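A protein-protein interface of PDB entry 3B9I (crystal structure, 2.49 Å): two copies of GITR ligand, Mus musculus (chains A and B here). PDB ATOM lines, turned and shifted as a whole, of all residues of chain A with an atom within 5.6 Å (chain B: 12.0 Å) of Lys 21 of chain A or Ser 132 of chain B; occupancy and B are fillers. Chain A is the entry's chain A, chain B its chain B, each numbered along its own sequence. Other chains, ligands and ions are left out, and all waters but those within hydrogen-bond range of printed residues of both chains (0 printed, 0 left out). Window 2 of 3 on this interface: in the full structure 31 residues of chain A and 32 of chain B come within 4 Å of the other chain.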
ATOM      1  N   LYS A  14      -1.902  -2.217  -5.106  1.00  0.00           N
ATOM      2  CA  LYS A  14      -2.271  -3.302  -4.209  1.00  0.00           C
ATOM      3  C   LYS A  14      -1.012  -3.892  -3.607  1.00  0.00           C
ATOM      4  O   LYS A  14      -0.156  -4.398  -4.326  1.00  0.00           O
ATOM      5  CB  LYS A  14      -3.045  -4.394  -4.936  1.00  0.00           C
ATOM      6  CG  LYS A  14      -3.672  -5.420  -3.984  1.00  0.00           C
ATOM      7  CD  LYS A  14      -3.605  -6.847  -4.551  1.00  0.00           C
ATOM      8  CE  LYS A  14      -4.951  -7.296  -5.080  1.00  0.00           C
ATOM      9  NZ  LYS A  14      -4.804  -8.077  -6.346  1.00  0.00           N
ATOM     10  N   PHE A  15      -0.914  -3.824  -2.286  1.00  0.00           N
ATOM     11  CA  PHE A  15       0.240  -4.318  -1.556  1.00  0.00           C
ATOM     12  C   PHE A  15      -0.084  -5.680  -0.966  1.00  0.00           C
ATOM     13  O   PHE A  15      -1.020  -5.788  -0.187  1.00  0.00           O
ATOM     14  CB  PHE A  15       0.570  -3.338  -0.422  1.00  0.00           C
ATOM     15  CG  PHE A  15       1.784  -3.704   0.356  1.00  0.00           C
ATOM     16  CD1 PHE A  15       3.053  -3.561  -0.202  1.00  0.00           C
ATOM     17  CD2 PHE A  15       1.671  -4.206   1.650  1.00  0.00           C
ATOM     18  CE1 PHE A  15       4.195  -3.903   0.533  1.00  0.00           C
ATOM     19  CE2 PHE A  15       2.803  -4.549   2.386  1.00  0.00           C
ATOM     20  CZ  PHE A  15       4.066  -4.398   1.831  1.00  0.00           C
ATOM     21  N   GLU A  16       0.670  -6.714  -1.339  1.00  0.00           N
ATOM     22  CA  GLU A  16       0.515  -8.043  -0.726  1.00  0.00           C
ATOM     23  C   GLU A  16       1.586  -8.203   0.343  1.00  0.00           C
ATOM     24  O   GLU A  16       2.785  -8.136   0.051  1.00  0.00           O
ATOM     25  CB  GLU A  16       0.630  -9.189  -1.750  1.00  0.00           C
ATOM     26  CG  GLU A  16      -0.273  -9.102  -3.005  1.00  0.00           C
ATOM     27  CD  GLU A  16      -1.648  -9.844  -2.910  1.00  0.00           C
ATOM     28  OE1 GLU A  16      -1.983 -10.481  -1.872  1.00  0.00           O
ATOM     29  OE2 GLU A  16      -2.409  -9.781  -3.910  1.00  0.00           O
ATOM     30  N   SER A  19       4.694 -11.007   0.165  1.00  0.00           N
ATOM     31  CA  SER A  19       5.868 -10.757  -0.655  1.00  0.00           C
ATOM     32  C   SER A  19       6.422  -9.350  -0.450  1.00  0.00           C
ATOM     33  O   SER A  19       7.538  -9.046  -0.856  1.00  0.00           O
ATOM     34  CB  SER A  19       5.513 -10.985  -2.135  1.00  0.00           C
ATOM     35  OG  SER A  19       4.310 -10.315  -2.477  1.00  0.00           O
ATOM     36  N   SER A  20       5.629  -8.485   0.173  1.00  0.00           N
ATOM     37  CA  SER A  20       6.013  -7.088   0.356  1.00  0.00           C
ATOM     38  C   SER A  20       6.172  -6.326  -0.945  1.00  0.00           C
ATOM     39  O   SER A  20       6.990  -5.423  -1.042  1.00  0.00           O
ATOM     40  CB  SER A  20       7.291  -6.978   1.183  1.00  0.00           C
ATOM     41  OG  SER A  20       6.976  -6.537   2.490  1.00  0.00           O
ATOM     42  N   LYS A  21       5.370  -6.679  -1.940  1.00  0.00           N
ATOM     43  CA  LYS A  21       5.427  -6.017  -3.233  1.00  0.00           C
ATOM     44  C   LYS A  21       4.131  -5.304  -3.506  1.00  0.00           C
ATOM     45  O   LYS A  21       3.072  -5.761  -3.095  1.00  0.00           O
ATOM     46  CB  LYS A  21       5.699  -7.035  -4.355  1.00  0.00           C
ATOM     47  CG  LYS A  21       7.094  -7.674  -4.262  1.00  0.00           C
ATOM     48  CD  LYS A  21       8.178  -6.597  -4.010  1.00  0.00           C
ATOM     49  CE  LYS A  21       9.593  -7.171  -4.030  1.00  0.00           C
ATOM     50  NZ  LYS A  21       9.752  -8.075  -5.211  1.00  0.00           N
ATOM     51  N   TRP A  22       4.225  -4.184  -4.211  1.00  0.00           N
ATOM     52  CA  TRP A  22       3.069  -3.470  -4.735  1.00  0.00           C
ATOM     53  C   TRP A  22       2.757  -3.925  -6.153  1.00  0.00           C
ATOM     54  O   TRP A  22       3.663  -4.167  -6.953  1.00  0.00           O
ATOM     55  CB  TRP A  22       3.352  -1.966  -4.746  1.00  0.00           C
ATOM     56  CG  TRP A  22       3.355  -1.342  -3.380  1.00  0.00           C
ATOM     57  CD1 TRP A  22       4.442  -1.121  -2.593  1.00  0.00           C
ATOM     58  CD2 TRP A  22       2.213  -0.864  -2.634  1.00  0.00           C
ATOM     59  NE1 TRP A  22       4.056  -0.532  -1.403  1.00  0.00           N
ATOM     60  CE2 TRP A  22       2.696  -0.366  -1.404  1.00  0.00           C
ATOM     61  CE3 TRP A  22       0.826  -0.818  -2.890  1.00  0.00           C
ATOM     62  CZ2 TRP A  22       1.855   0.182  -0.425  1.00  0.00           C
ATOM     63  CZ3 TRP A  22      -0.022  -0.274  -1.912  1.00  0.00           C
ATOM     64  CH2 TRP A  22       0.505   0.210  -0.686  1.00  0.00           C
ATOM     65  N   HIS A  23       1.477  -4.062  -6.463  1.00  0.00           N
ATOM     66  CA  HIS A  23       1.046  -4.186  -7.859  1.00  0.00           C
ATOM     67  C   HIS A  23       0.283  -2.932  -8.231  1.00  0.00           C
ATOM     68  O   HIS A  23      -0.472  -2.409  -7.421  1.00  0.00           O
ATOM     69  CB  HIS A  23       0.207  -5.445  -8.076  1.00  0.00           C
ATOM     70  CG  HIS A  23       0.876  -6.681  -7.570  1.00  0.00           C
ATOM     71  ND1 HIS A  23       1.427  -7.625  -8.408  1.00  0.00           N
ATOM     72  CD2 HIS A  23       1.140  -7.095  -6.307  1.00  0.00           C
ATOM     73  CE1 HIS A  23       1.974  -8.584  -7.684  1.00  0.00           C
ATOM     74  NE2 HIS A  23       1.814  -8.286  -6.406  1.00  0.00           N
ATOM     75  N   MET A  24       0.507  -2.435  -9.444  1.00  0.00           N
ATOM     76  CA  MET A  24       0.003  -1.122  -9.825  1.00  0.00           C
ATOM     77  C   MET A  24      -0.505  -1.045 -11.262  1.00  0.00           C
ATOM     78  O   MET A  24      -0.064  -1.794 -12.145  1.00  0.00           O
ATOM     79  CB  MET A  24       1.097  -0.095  -9.613  1.00  0.00           C
ATOM     80  CG  MET A  24       2.029  -0.486  -8.506  1.00  0.00           C
ATOM     81  SD  MET A  24       3.341   0.691  -8.256  1.00  0.00           S
ATOM     82  CE  MET A  24       4.502   0.206  -9.541  1.00  0.00           C
ATOM     83  N   THR A  34       4.709   4.753  -3.402  1.00  0.00           N
ATOM     84  CA  THR A  34       4.606   3.668  -2.452  1.00  0.00           C
ATOM     85  C   THR A  34       5.975   3.363  -1.863  1.00  0.00           C
ATOM     86  O   THR A  34       7.015   3.718  -2.441  1.00  0.00           O
ATOM     87  CB  THR A  34       4.077   2.392  -3.107  1.00  0.00           C
ATOM     88  OG1 THR A  34       5.067   1.894  -4.008  1.00  0.00           O
ATOM     89  CG2 THR A  34       2.773   2.648  -3.860  1.00  0.00           C
ATOM     90  N   LEU B 128      -3.393  -5.072 -12.608  1.00  0.00           N
ATOM     91  CA  LEU B 128      -2.288  -4.419 -11.929  1.00  0.00           C
ATOM     92  C   LEU B 128      -1.025  -5.138 -12.345  1.00  0.00           C
ATOM     93  O   LEU B 128      -0.490  -5.943 -11.577  1.00  0.00           O
ATOM     94  CB  LEU B 128      -2.476  -4.476 -10.408  1.00  0.00           C
ATOM     95  CG  LEU B 128      -3.831  -3.945  -9.926  1.00  0.00           C
ATOM     96  CD1 LEU B 128      -4.142  -4.427  -8.540  1.00  0.00           C
ATOM     97  CD2 LEU B 128      -3.891  -2.398 -10.017  1.00  0.00           C
ATOM     98  N   PRO B 129      -0.548  -4.865 -13.574  1.00  0.00           N
ATOM     99  CA  PRO B 129       0.572  -5.635 -14.101  1.00  0.00           C
ATOM    100  C   PRO B 129       1.942  -5.181 -13.585  1.00  0.00           C
ATOM    101  O   PRO B 129       2.909  -5.914 -13.751  1.00  0.00           O
ATOM    102  CB  PRO B 129       0.483  -5.405 -15.622  1.00  0.00           C
ATOM    103  CG  PRO B 129      -0.626  -4.382 -15.857  1.00  0.00           C
ATOM    104  CD  PRO B 129      -0.988  -3.822 -14.521  1.00  0.00           C
ATOM    105  N   PHE B 130       2.039  -4.010 -12.963  1.00  0.00           N
ATOM    106  CA  PHE B 130       3.367  -3.478 -12.632  1.00  0.00           C
ATOM    107  C   PHE B 130       3.742  -3.678 -11.185  1.00  0.00           C
ATOM    108  O   PHE B 130       3.017  -3.270 -10.280  1.00  0.00           O
ATOM    109  CB  PHE B 130       3.524  -2.017 -13.071  1.00  0.00           C
ATOM    110  CG  PHE B 130       3.342  -1.829 -14.541  1.00  0.00           C
ATOM    111  CD1 PHE B 130       4.374  -2.135 -15.427  1.00  0.00           C
ATOM    112  CD2 PHE B 130       2.122  -1.414 -15.055  1.00  0.00           C
ATOM    113  CE1 PHE B 130       4.196  -1.987 -16.805  1.00  0.00           C
ATOM    114  CE2 PHE B 130       1.944  -1.261 -16.417  1.00  0.00           C
ATOM    115  CZ  PHE B 130       2.979  -1.550 -17.297  1.00  0.00           C
ATOM    116  N   ILE B 131       4.903  -4.294 -10.996  1.00  0.00           N
ATOM    117  CA  ILE B 131       5.271  -4.934  -9.739  1.00  0.00           C
ATOM    118  C   ILE B 131       6.451  -4.253  -9.067  1.00  0.00           C
ATOM    119  O   ILE B 131       7.046  -3.331  -9.615  1.00  0.00           O
ATOM    120  CB  ILE B 131       5.513  -6.465  -9.955  1.00  0.00           C
ATOM    121  CG1 ILE B 131       4.181  -7.164 -10.272  1.00  0.00           C
ATOM    122  CG2 ILE B 131       6.183  -7.134  -8.750  1.00  0.00           C
ATOM    123  CD1 ILE B 131       4.250  -8.714 -10.290  1.00  0.00           C
ATOM    124  N   SER B 132       6.754  -4.736  -7.867  1.00  0.00           N
ATOM    125  CA  SER B 132       7.711  -4.160  -6.912  1.00  0.00           C
ATOM    126  C   SER B 132       7.154  -2.913  -6.254  1.00  0.00           C
ATOM    127  O   SER B 132       6.992  -2.879  -5.033  1.00  0.00           O
ATOM    128  CB  SER B 132       9.075  -3.885  -7.536  1.00  0.00           C
ATOM    129  OG  SER B 132      10.090  -3.941  -6.550  1.00  0.00           O
ATOM    130  OXT SER B 132       6.844  -1.943  -6.940  1.00  0.00           O
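Of the 10 printed residues of chain A, 5 touch a printed residue of chain B.
Of the 5 printed residues of chain B, 5 touch a printed residue of chain A.
Hydrophobic or aromatic side chains of chain B that line the printed part of chain A: Leu 128, Pro 129, Phe 130 and Ile 131.
Among the printed residues, 11 pairs touch across the chains.
Among the printed residues, no Asp or Glu carboxylate lies within 4 Å of a Lys or Arg side-chain nitrogen of the other chain.
No residue of chain B comes within 4 Å of Phe 15 of chain A.
No residue of chain B comes within 4 Å of Glu 16 of chain A.
No residue of chain B comes within 4 Å of Ser 19 of chain A.
No residue of chain B comes within 4 Å of Ser 20 of chain A.
His 23 of chain A touches just these residues of chain B: Leu 128 (3.6 Å), Phe 130 (3.3 Å) and Ile 131 (3.4 Å).
Printed residues of chain B within 4 Å of Met 24 of chain A: Leu 128, Pro 129 and Phe 130.
Thr 34 of chain A touches none of the printed residues of chain B.
Of the printed residues of chain A, Leu 128 of chain B touches Lys 14 (3.8 Å), His 23 (3.6 Å) and Met 24 (3.4 Å).
Of the printed residues of chain A, Phe 130 of chain B touches Trp 22 (3.5 Å), His 23 (3.3 Å) and Met 24 (2.8 Å).
Of the printed residues of chain A, Ile 131 of chain B touches Trp 22 (3.3 Å) and His 23 (3.4 Å).
Of chain A, only Lys 21 (3.8 Å) and Trp 22 (3.2 Å) come within 4 Å of Ser 132 of chain B.
The nearest residue of chain A that does not touch Ser 132 of chain B is Met 24 of chain A (4.1 Å).
The backbone carbonyl oxygen (O) of Phe 130 of chain B is in hydrogen-bond range of the backbone NH (N) of Met 24 of chain A, 2.8 Å away.
N of Trp 22 of chain A sits at hydrogen-bond distance from O of Ser 132 of chain B (3.2 Å).
O of Met 24 of chain A sits close to N of Pro 129 of chain B (3.4 Å).
Leu 128 of chain B touches Lys 14 of chain A.
Lys 21 of chain A touches Ser 132 of chain B (CD to CA, 3.8 Å).
Trp 22 of chain A touches Phe 130 of chain B.
Trp 22 of chain A touches Ile 131 of chain B.
CB of His 23 of chain A touches O of Leu 128 of chain B (3.6 Å).
His 23 of chain A touches Phe 130 of chain B.
CG1 of Ile 131 of chain B touches ND1 of His 23 of chain A (3.4 Å).
Leu 128 of chain B touches Met 24 of chain A (CA to O, 3.4 Å).
The backbone carbonyl oxygen (O) of Lys 14 of chain A is in hydrogen-bond range of the backbone NH (N) of His 23 of chain A, at 2.7 Å.
The backbone NH (N) of Glu 16 of chain A lies within hydrogen-bond range of the backbone carbonyl oxygen (O) of Lys 21 of chain A, 3.1 Å away.
The side-chain amino group (NZ) of Lys 14 of chain A lies within salt-bridge range of the side-chain carboxylate (OE2) of Glu 16 of chain A (3.8 Å).
No position is printed for both chains.
Of the 11 pairs that touch across the chains among the printed residues, none has its exchanged pair printed and touching as well.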
